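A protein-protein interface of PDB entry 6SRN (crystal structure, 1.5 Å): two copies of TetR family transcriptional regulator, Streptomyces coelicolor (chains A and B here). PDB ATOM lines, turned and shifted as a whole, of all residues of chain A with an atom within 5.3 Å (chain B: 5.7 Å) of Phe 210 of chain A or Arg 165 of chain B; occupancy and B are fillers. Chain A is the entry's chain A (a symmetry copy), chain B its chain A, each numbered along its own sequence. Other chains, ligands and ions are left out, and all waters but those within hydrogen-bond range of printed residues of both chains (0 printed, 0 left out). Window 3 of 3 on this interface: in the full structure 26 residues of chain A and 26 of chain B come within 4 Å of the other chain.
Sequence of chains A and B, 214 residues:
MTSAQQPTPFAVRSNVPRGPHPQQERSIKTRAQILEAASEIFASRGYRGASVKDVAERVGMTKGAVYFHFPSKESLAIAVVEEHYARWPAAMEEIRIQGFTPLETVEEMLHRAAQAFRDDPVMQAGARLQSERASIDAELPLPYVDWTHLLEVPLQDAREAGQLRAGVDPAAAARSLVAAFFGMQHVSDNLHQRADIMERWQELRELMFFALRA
NE of Arg 165 of chain B lies within hydrogen-bond range of O of Ala 211 of chain B, at 2.8 Å.
The backbone carbonyl oxygen (O) of Leu 212 of chain B sits at hydrogen-bond distance from the backbone NH (N) of Arg 165 of chain B (2.9 Å).
Arg 165 of chain B touches Leu 207 of chain A (NH2 to CD2, 3.7 Å).
Ala 211 of chain B touches Leu 207 of chain A.
CD2 of Leu 207 of chain A touches CD2 of Leu 212 of chain B, 3.96 Å away.
Arg 165 of chain B touches Phe 210 of chain A.
Phe 210 of chain B touches Phe 210 of chain A (CE1 to CE1, 3.9 Å).
CD1 of Phe 210 of chain A touches CA of Ala 211 of chain B, at 3.9 Å.
Ala 211 of chain A touches Phe 210 of chain B.
Phe 210 of chain B touches its own counterpart, Phe 210 of chain A.
Phe 210 of chain A touches Ala 211 of chain B, and with the chains exchanged Ala 211 of chain A touches Phe 210 of chain B.
Positions printed for both chains: 210, 211, 212 and 213.
Of the 8 pairs that touch across the chains among the printed residues, 3 have their exchanged pair printed and touching as well.
The side-chain carboxylate of Glu 206 of chain A lies within salt-bridge range of the guanidinium group of Arg 165 of chain B, 3.0 Å away.
Phe 210 of chain A touches three residues of chain B.
Of the printed residues of chain A, Arg 165 of chain B touches Glu 206, Leu 207 and Phe 210.
Of the printed residues of chain B, Leu 207 of chain A touches Arg 165 (3.7 Å), Ala 211 (3.2 Å) and Leu 212 (3.96 Å).
Printed residues of chain B within 4 Å of Glu 206 of chain A: Arg 165 (3.0 Å).
Printed residues of chain A within 4 Å of Ala 211 of chain B: Leu 207 (3.2 Å) and Phe 210 (3.9 Å).
Of the printed residues of chain A, Phe 210 of chain B touches Phe 210 and Ala 211.
The nearest printed residue of chain B that does not touch Phe 210 of chain A is Arg 213 of chain B (6.0 Å).
The nearest printed residue of chain A that does not touch Arg 165 of chain B is Ala 211 of chain A (6.5 Å).
Printed residues of chain A that touch a printed residue of chain B: Glu 206, Leu 207, Phe 210 and Ala 211.
Hydrophobic or aromatic side chains of chain A that line the printed part of chain B: Leu 207 and Phe 210.
Among the printed residues, 8 pairs touch across the chains.
Among the printed residues, Asp or Glu carboxylates within 4 Å of a Lys or Arg side-chain nitrogen of the other chain: Glu 206 of chain A with Arg 165 of chain B.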
ATOM      1  N   ARG A 205      10.355 -18.560  11.728  1.00  0.00           N
ATOM      2  CA  ARG A 205      10.444 -19.689  10.780  1.00  0.00           C
ATOM      3  C   ARG A 205      10.264 -19.190   9.351  1.00  0.00           C
ATOM      4  O   ARG A 205      10.987 -19.624   8.417  1.00  0.00           O
ATOM      5  CB  ARG A 205       9.340 -20.634  11.181  1.00  0.00           C
ATOM      6  CG  ARG A 205       9.006 -21.885  10.466  1.00  0.00           C
ATOM      7  CD  ARG A 205       7.611 -22.138  11.024  1.00  0.00           C
ATOM      8  NE  ARG A 205       6.607 -21.968  10.008  1.00  0.00           N
ATOM      9  CZ  ARG A 205       6.511 -22.760   8.955  1.00  0.00           C
ATOM     10  NH1 ARG A 205       7.382 -23.760   8.775  1.00  0.00           N
ATOM     11  NH2 ARG A 205       5.552 -22.564   8.085  1.00  0.00           N
ATOM     12  N   GLU A 206       9.358 -18.246   9.142  1.00  0.00           N
ATOM     13  CA  GLU A 206       9.160 -17.739   7.777  1.00  0.00           C
ATOM     14  C   GLU A 206      10.464 -17.156   7.220  1.00  0.00           C
ATOM     15  O   GLU A 206      10.849 -17.415   6.047  1.00  0.00           O
ATOM     16  CB  GLU A 206       7.997 -16.738   7.725  1.00  0.00           C
ATOM     17  CG  GLU A 206       7.568 -16.385   6.295  1.00  0.00           C
ATOM     18  CD  GLU A 206       8.432 -15.363   5.582  1.00  0.00           C
ATOM     19  OE1 GLU A 206       9.126 -14.513   6.204  1.00  0.00           O
ATOM     20  OE2 GLU A 206       8.372 -15.366   4.309  1.00  0.00           O
ATOM     21  N   LEU A 207      11.167 -16.405   8.043  1.00  0.00           N
ATOM     22  CA  LEU A 207      12.453 -15.870   7.606  1.00  0.00           C
ATOM     23  C   LEU A 207      13.497 -16.974   7.414  1.00  0.00           C
ATOM     24  O   LEU A 207      14.189 -17.029   6.401  1.00  0.00           O
ATOM     25  CB  LEU A 207      12.992 -14.895   8.646  1.00  0.00           C
ATOM     26  CG  LEU A 207      12.149 -13.674   8.980  1.00  0.00           C
ATOM     27  CD1 LEU A 207      12.803 -12.891  10.111  1.00  0.00           C
ATOM     28  CD2 LEU A 207      11.962 -12.796   7.766  1.00  0.00           C
ATOM     29  N   MET A 208      13.622 -17.869   8.387  1.00  0.00           N
ATOM     30  CA  MET A 208      14.684 -18.875   8.319  1.00  0.00           C
ATOM     31  C   MET A 208      14.481 -19.776   7.138  1.00  0.00           C
ATOM     32  O   MET A 208      15.443 -20.055   6.438  1.00  0.00           O
ATOM     33  CB  MET A 208      14.725 -19.687   9.600  1.00  0.00           C
ATOM     34  CG  MET A 208      14.936 -18.753  10.760  1.00  0.00           C
ATOM     35  SD  MET A 208      16.639 -18.294  10.951  1.00  0.00           S
ATOM     36  CE  MET A 208      17.516 -19.832  11.387  1.00  0.00           C
ATOM     37  N   PHE A 209      13.266 -20.260   6.921  1.00  0.00           N
ATOM     38  CA  PHE A 209      13.048 -21.183   5.804  1.00  0.00           C
ATOM     39  C   PHE A 209      13.046 -20.482   4.451  1.00  0.00           C
ATOM     40  O   PHE A 209      13.467 -21.097   3.480  1.00  0.00           O
ATOM     41  CB  PHE A 209      11.839 -22.065   6.044  1.00  0.00           C
ATOM     42  CG  PHE A 209      12.117 -23.124   7.041  1.00  0.00           C
ATOM     43  CD1 PHE A 209      12.711 -24.335   6.680  1.00  0.00           C
ATOM     44  CD2 PHE A 209      11.904 -22.860   8.376  1.00  0.00           C
ATOM     45  CE1 PHE A 209      13.032 -25.281   7.656  1.00  0.00           C
ATOM     46  CE2 PHE A 209      12.201 -23.812   9.323  1.00  0.00           C
ATOM     47  CZ  PHE A 209      12.785 -24.993   8.974  1.00  0.00           C
ATOM     48  N   PHE A 210      12.709 -19.202   4.411  1.00  0.00           N
ATOM     49  CA  PHE A 210      12.872 -18.417   3.171  1.00  0.00           C
ATOM     50  C   PHE A 210      14.344 -18.404   2.769  1.00  0.00           C
ATOM     51  O   PHE A 210      14.686 -18.571   1.563  1.00  0.00           O
ATOM     52  CB  PHE A 210      12.366 -16.999   3.319  1.00  0.00           C
ATOM     53  CG  PHE A 210      12.515 -16.193   2.069  1.00  0.00           C
ATOM     54  CD1 PHE A 210      13.690 -15.496   1.803  1.00  0.00           C
ATOM     55  CD2 PHE A 210      11.485 -16.155   1.168  1.00  0.00           C
ATOM     56  CE1 PHE A 210      13.823 -14.761   0.634  1.00  0.00           C
ATOM     57  CE2 PHE A 210      11.604 -15.433   0.001  1.00  0.00           C
ATOM     58  CZ  PHE A 210      12.781 -14.753  -0.272  1.00  0.00           C
ATOM     59  N   ALA A 211      15.207 -18.287   3.775  1.00  0.00           N
ATOM     60  CA  ALA A 211      16.660 -18.258   3.561  1.00  0.00           C
ATOM     61  C   ALA A 211      17.280 -19.625   3.276  1.00  0.00           C
ATOM     62  O   ALA A 211      18.383 -19.696   2.728  1.00  0.00           O
ATOM     63  CB  ALA A 211      17.316 -17.615   4.748  1.00  0.00           C
ATOM     64  N   LEU A 212      16.626 -20.717   3.672  1.00  0.00           N
ATOM     65  CA  LEU A 212      17.151 -22.062   3.476  1.00  0.00           C
ATOM     66  C   LEU A 212      16.714 -22.655   2.152  1.00  0.00           C
ATOM     67  O   LEU A 212      17.417 -23.468   1.585  1.00  0.00           O
ATOM     68  CB  LEU A 212      16.739 -23.027   4.587  1.00  0.00           C
ATOM     69  CG  LEU A 212      17.386 -22.677   5.927  1.00  0.00           C
ATOM     70  CD1 LEU A 212      16.684 -23.466   6.998  1.00  0.00           C
ATOM     71  CD2 LEU A 212      18.867 -22.971   5.946  1.00  0.00           C
ATOM     72  N   ARG A 213      15.514 -22.336   1.708  1.00  0.00           N
ATOM     73  CA  ARG A 213      14.997 -22.976   0.471  1.00  0.00           C
ATOM     74  C   ARG A 213      15.656 -22.488  -0.806  1.00  0.00           C
ATOM     75  O   ARG A 213      15.765 -21.283  -1.079  1.00  0.00           O
ATOM     76  CB  ARG A 213      13.520 -22.699   0.307  1.00  0.00           C
ATOM     77  CG  ARG A 213      12.635 -23.430   1.256  1.00  0.00           C
ATOM     78  CD  ARG A 213      11.199 -23.283   0.768  1.00  0.00           C
ATOM     79  NE  ARG A 213      10.960 -21.937   0.260  1.00  0.00           N
ATOM     80  CZ  ARG A 213      10.510 -20.917   0.987  1.00  0.00           C
ATOM     81  NH1 ARG A 213      10.218 -21.064   2.304  1.00  0.00           N
ATOM     82  NH2 ARG A 213      10.346 -19.745   0.376  1.00  0.00           N
ATOM     83  N   GLN B 163      13.754  -1.200   1.512  1.00  0.00           N
ATOM     84  CA  GLN B 163      14.919  -2.035   1.739  1.00  0.00           C
ATOM     85  C   GLN B 163      14.536  -3.435   2.213  1.00  0.00           C
ATOM     86  O   GLN B 163      15.285  -4.417   2.074  1.00  0.00           O
ATOM     87  CB  GLN B 163      15.788  -1.306   2.782  1.00  0.00           C
ATOM     88  CG  GLN B 163      17.132  -1.929   3.005  1.00  0.00           C
ATOM     89  CD  GLN B 163      18.071  -1.050   3.817  1.00  0.00           C
ATOM     90  OE1 GLN B 163      17.683  -0.314   4.738  1.00  0.00           O
ATOM     91  NE2 GLN B 163      19.331  -1.129   3.464  1.00  0.00           N
ATOM     92  N   LEU B 164      13.359  -3.516   2.816  1.00  0.00           N
ATOM     93  CA  LEU B 164      12.915  -4.721   3.507  1.00  0.00           C
ATOM     94  C   LEU B 164      12.014  -5.486   2.537  1.00  0.00           C
ATOM     95  O   LEU B 164      11.177  -4.886   1.833  1.00  0.00           O
ATOM     96  CB  LEU B 164      12.201  -4.300   4.786  1.00  0.00           C
ATOM     97  CG  LEU B 164      12.159  -5.131   6.042  1.00  0.00           C
ATOM     98  CD1 LEU B 164      13.574  -5.289   6.582  1.00  0.00           C
ATOM     99  CD2 LEU B 164      11.266  -4.460   7.058  1.00  0.00           C
ATOM    100  N   ARG B 165      12.205  -6.794   2.415  1.00  0.00           N
ATOM    101  CA  ARG B 165      11.373  -7.641   1.553  1.00  0.00           C
ATOM    102  C   ARG B 165       9.865  -7.433   1.799  1.00  0.00           C
ATOM    103  O   ARG B 165       9.413  -7.277   2.941  1.00  0.00           O
ATOM    104  CB  ARG B 165      11.745  -9.143   1.671  1.00  0.00           C
ATOM    105  CG  ARG B 165      10.813 -10.144   0.984  1.00  0.00           C
ATOM    106  CD  ARG B 165      11.379 -11.566   0.946  1.00  0.00           C
ATOM    107  NE  ARG B 165      11.615 -12.084   2.296  1.00  0.00           N
ATOM    108  CZ  ARG B 165      10.790 -12.858   3.008  1.00  0.00           C
ATOM    109  NH1 ARG B 165       9.605 -13.264   2.572  1.00  0.00           N
ATOM    110  NH2 ARG B 165      11.141 -13.229   4.220  1.00  0.00           N
ATOM    111  N   ALA B 166       9.113  -7.441   0.698  1.00  0.00           N
ATOM    112  CA  ALA B 166       7.681  -7.209   0.731  1.00  0.00           C
ATOM    113  C   ALA B 166       7.007  -8.202   1.634  1.00  0.00           C
ATOM    114  O   ALA B 166       7.269  -9.419   1.584  1.00  0.00           O
ATOM    115  CB  ALA B 166       7.079  -7.286  -0.666  1.00  0.00           C
ATOM    116  N   GLY B 167       6.147  -7.660   2.488  1.00  0.00           N
ATOM    117  CA  GLY B 167       5.354  -8.461   3.385  1.00  0.00           C
ATOM    118  C   GLY B 167       5.984  -8.662   4.748  1.00  0.00           C
ATOM    119  O   GLY B 167       5.300  -9.103   5.670  1.00  0.00           O
ATOM    120  N   VAL B 168       7.287  -8.369   4.882  1.00  0.00           N
ATOM    121  CA  VAL B 168       7.938  -8.495   6.179  1.00  0.00           C
ATOM    122  C   VAL B 168       7.476  -7.382   7.113  1.00  0.00           C
ATOM    123  O   VAL B 168       7.539  -6.205   6.770  1.00  0.00           O
ATOM    124  CB  VAL B 168       9.473  -8.516   6.014  1.00  0.00           C
ATOM    125  CG1 VAL B 168      10.164  -8.540   7.372  1.00  0.00           C
ATOM    126  CG2 VAL B 168       9.874  -9.735   5.185  1.00  0.00           C
ATOM    127  N   PHE B 210      19.466 -12.390   4.704  1.00  0.00           N
ATOM    128  CA  PHE B 210      19.063 -12.826   3.353  1.00  0.00           C
ATOM    129  C   PHE B 210      17.544 -12.768   3.232  1.00  0.00           C
ATOM    130  O   PHE B 210      16.994 -12.300   2.195  1.00  0.00           O
ATOM    131  CB  PHE B 210      19.553 -14.220   3.030  1.00  0.00           C
ATOM    132  CG  PHE B 210      19.162 -14.673   1.661  1.00  0.00           C
ATOM    133  CD1 PHE B 210      17.942 -15.305   1.436  1.00  0.00           C
ATOM    134  CD2 PHE B 210      20.012 -14.448   0.611  1.00  0.00           C
ATOM    135  CE1 PHE B 210      17.583 -15.711   0.159  1.00  0.00           C
ATOM    136  CE2 PHE B 210      19.668 -14.842  -0.663  1.00  0.00           C
ATOM    137  CZ  PHE B 210      18.445 -15.454  -0.889  1.00  0.00           C
ATOM    138  N   ALA B 211      16.872 -13.167   4.311  1.00  0.00           N
ATOM    139  CA  ALA B 211      15.404 -13.173   4.362  1.00  0.00           C
ATOM    140  C   ALA B 211      14.776 -11.794   4.562  1.00  0.00           C
ATOM    141  O   ALA B 211      13.595 -11.609   4.259  1.00  0.00           O
ATOM    142  CB  ALA B 211      14.957 -14.121   5.436  1.00  0.00           C
ATOM    143  N   LEU B 212      15.517 -10.829   5.106  1.00  0.00           N
ATOM    144  CA  LEU B 212      14.998  -9.493   5.367  1.00  0.00           C
ATOM    145  C   LEU B 212      15.204  -8.563   4.189  1.00  0.00           C
ATOM    146  O   LEU B 212      14.430  -7.647   3.991  1.00  0.00           O
ATOM    147  CB  LEU B 212      15.626  -8.843   6.600  1.00  0.00           C
ATOM    148  CG  LEU B 212      15.222  -9.549   7.895  1.00  0.00           C
ATOM    149  CD1 LEU B 212      16.125  -9.051   8.991  1.00  0.00           C
ATOM    150  CD2 LEU B 212      13.777  -9.306   8.256  1.00  0.00           C
ATOM    151  N   ARG B 213      16.297  -8.725   3.469  1.00  0.00           N
ATOM    152  CA  ARG B 213      16.598  -7.771   2.371  1.00  0.00           C
ATOM    153  C   ARG B 213      15.709  -7.922   1.151  1.00  0.00           C
ATOM    154  O   ARG B 213      15.523  -9.016   0.595  1.00  0.00           O
ATOM    155  CB  ARG B 213      18.014  -7.959   1.877  1.00  0.00           C
ATOM    156  CG  ARG B 213      19.073  -7.482   2.809  1.00  0.00           C
ATOM    157  CD  ARG B 213      20.395  -7.461   2.050  1.00  0.00           C
ATOM    158  NE  ARG B 213      20.505  -8.620   1.173  1.00  0.00           N
ATOM    159  CZ  ARG B 213      21.054  -9.784   1.513  1.00  0.00           C
ATOM    160  NH1 ARG B 213      21.581  -9.980   2.748  1.00  0.00           N
ATOM    161  NH2 ARG B 213      21.078 -10.751   0.597  1.00  0.00           N
ATOM    162  N   ALA B 214      15.181  -6.802   0.689  1.00  0.00           N
ATOM    163  CA  ALA B 214      14.549  -6.769  -0.600  1.00  0.00           C
ATOM    164  C   ALA B 214      15.619  -7.062  -1.647  1.00  0.00           C
ATOM    165  O   ALA B 214      16.759  -6.550  -1.552  1.00  0.00           O
ATOM    166  CB  ALA B 214      13.930  -5.399  -0.840  1.00  0.00           C
ATOM    167  OXT ALA B 214      15.351  -7.833  -2.559  1.00  0.00           O
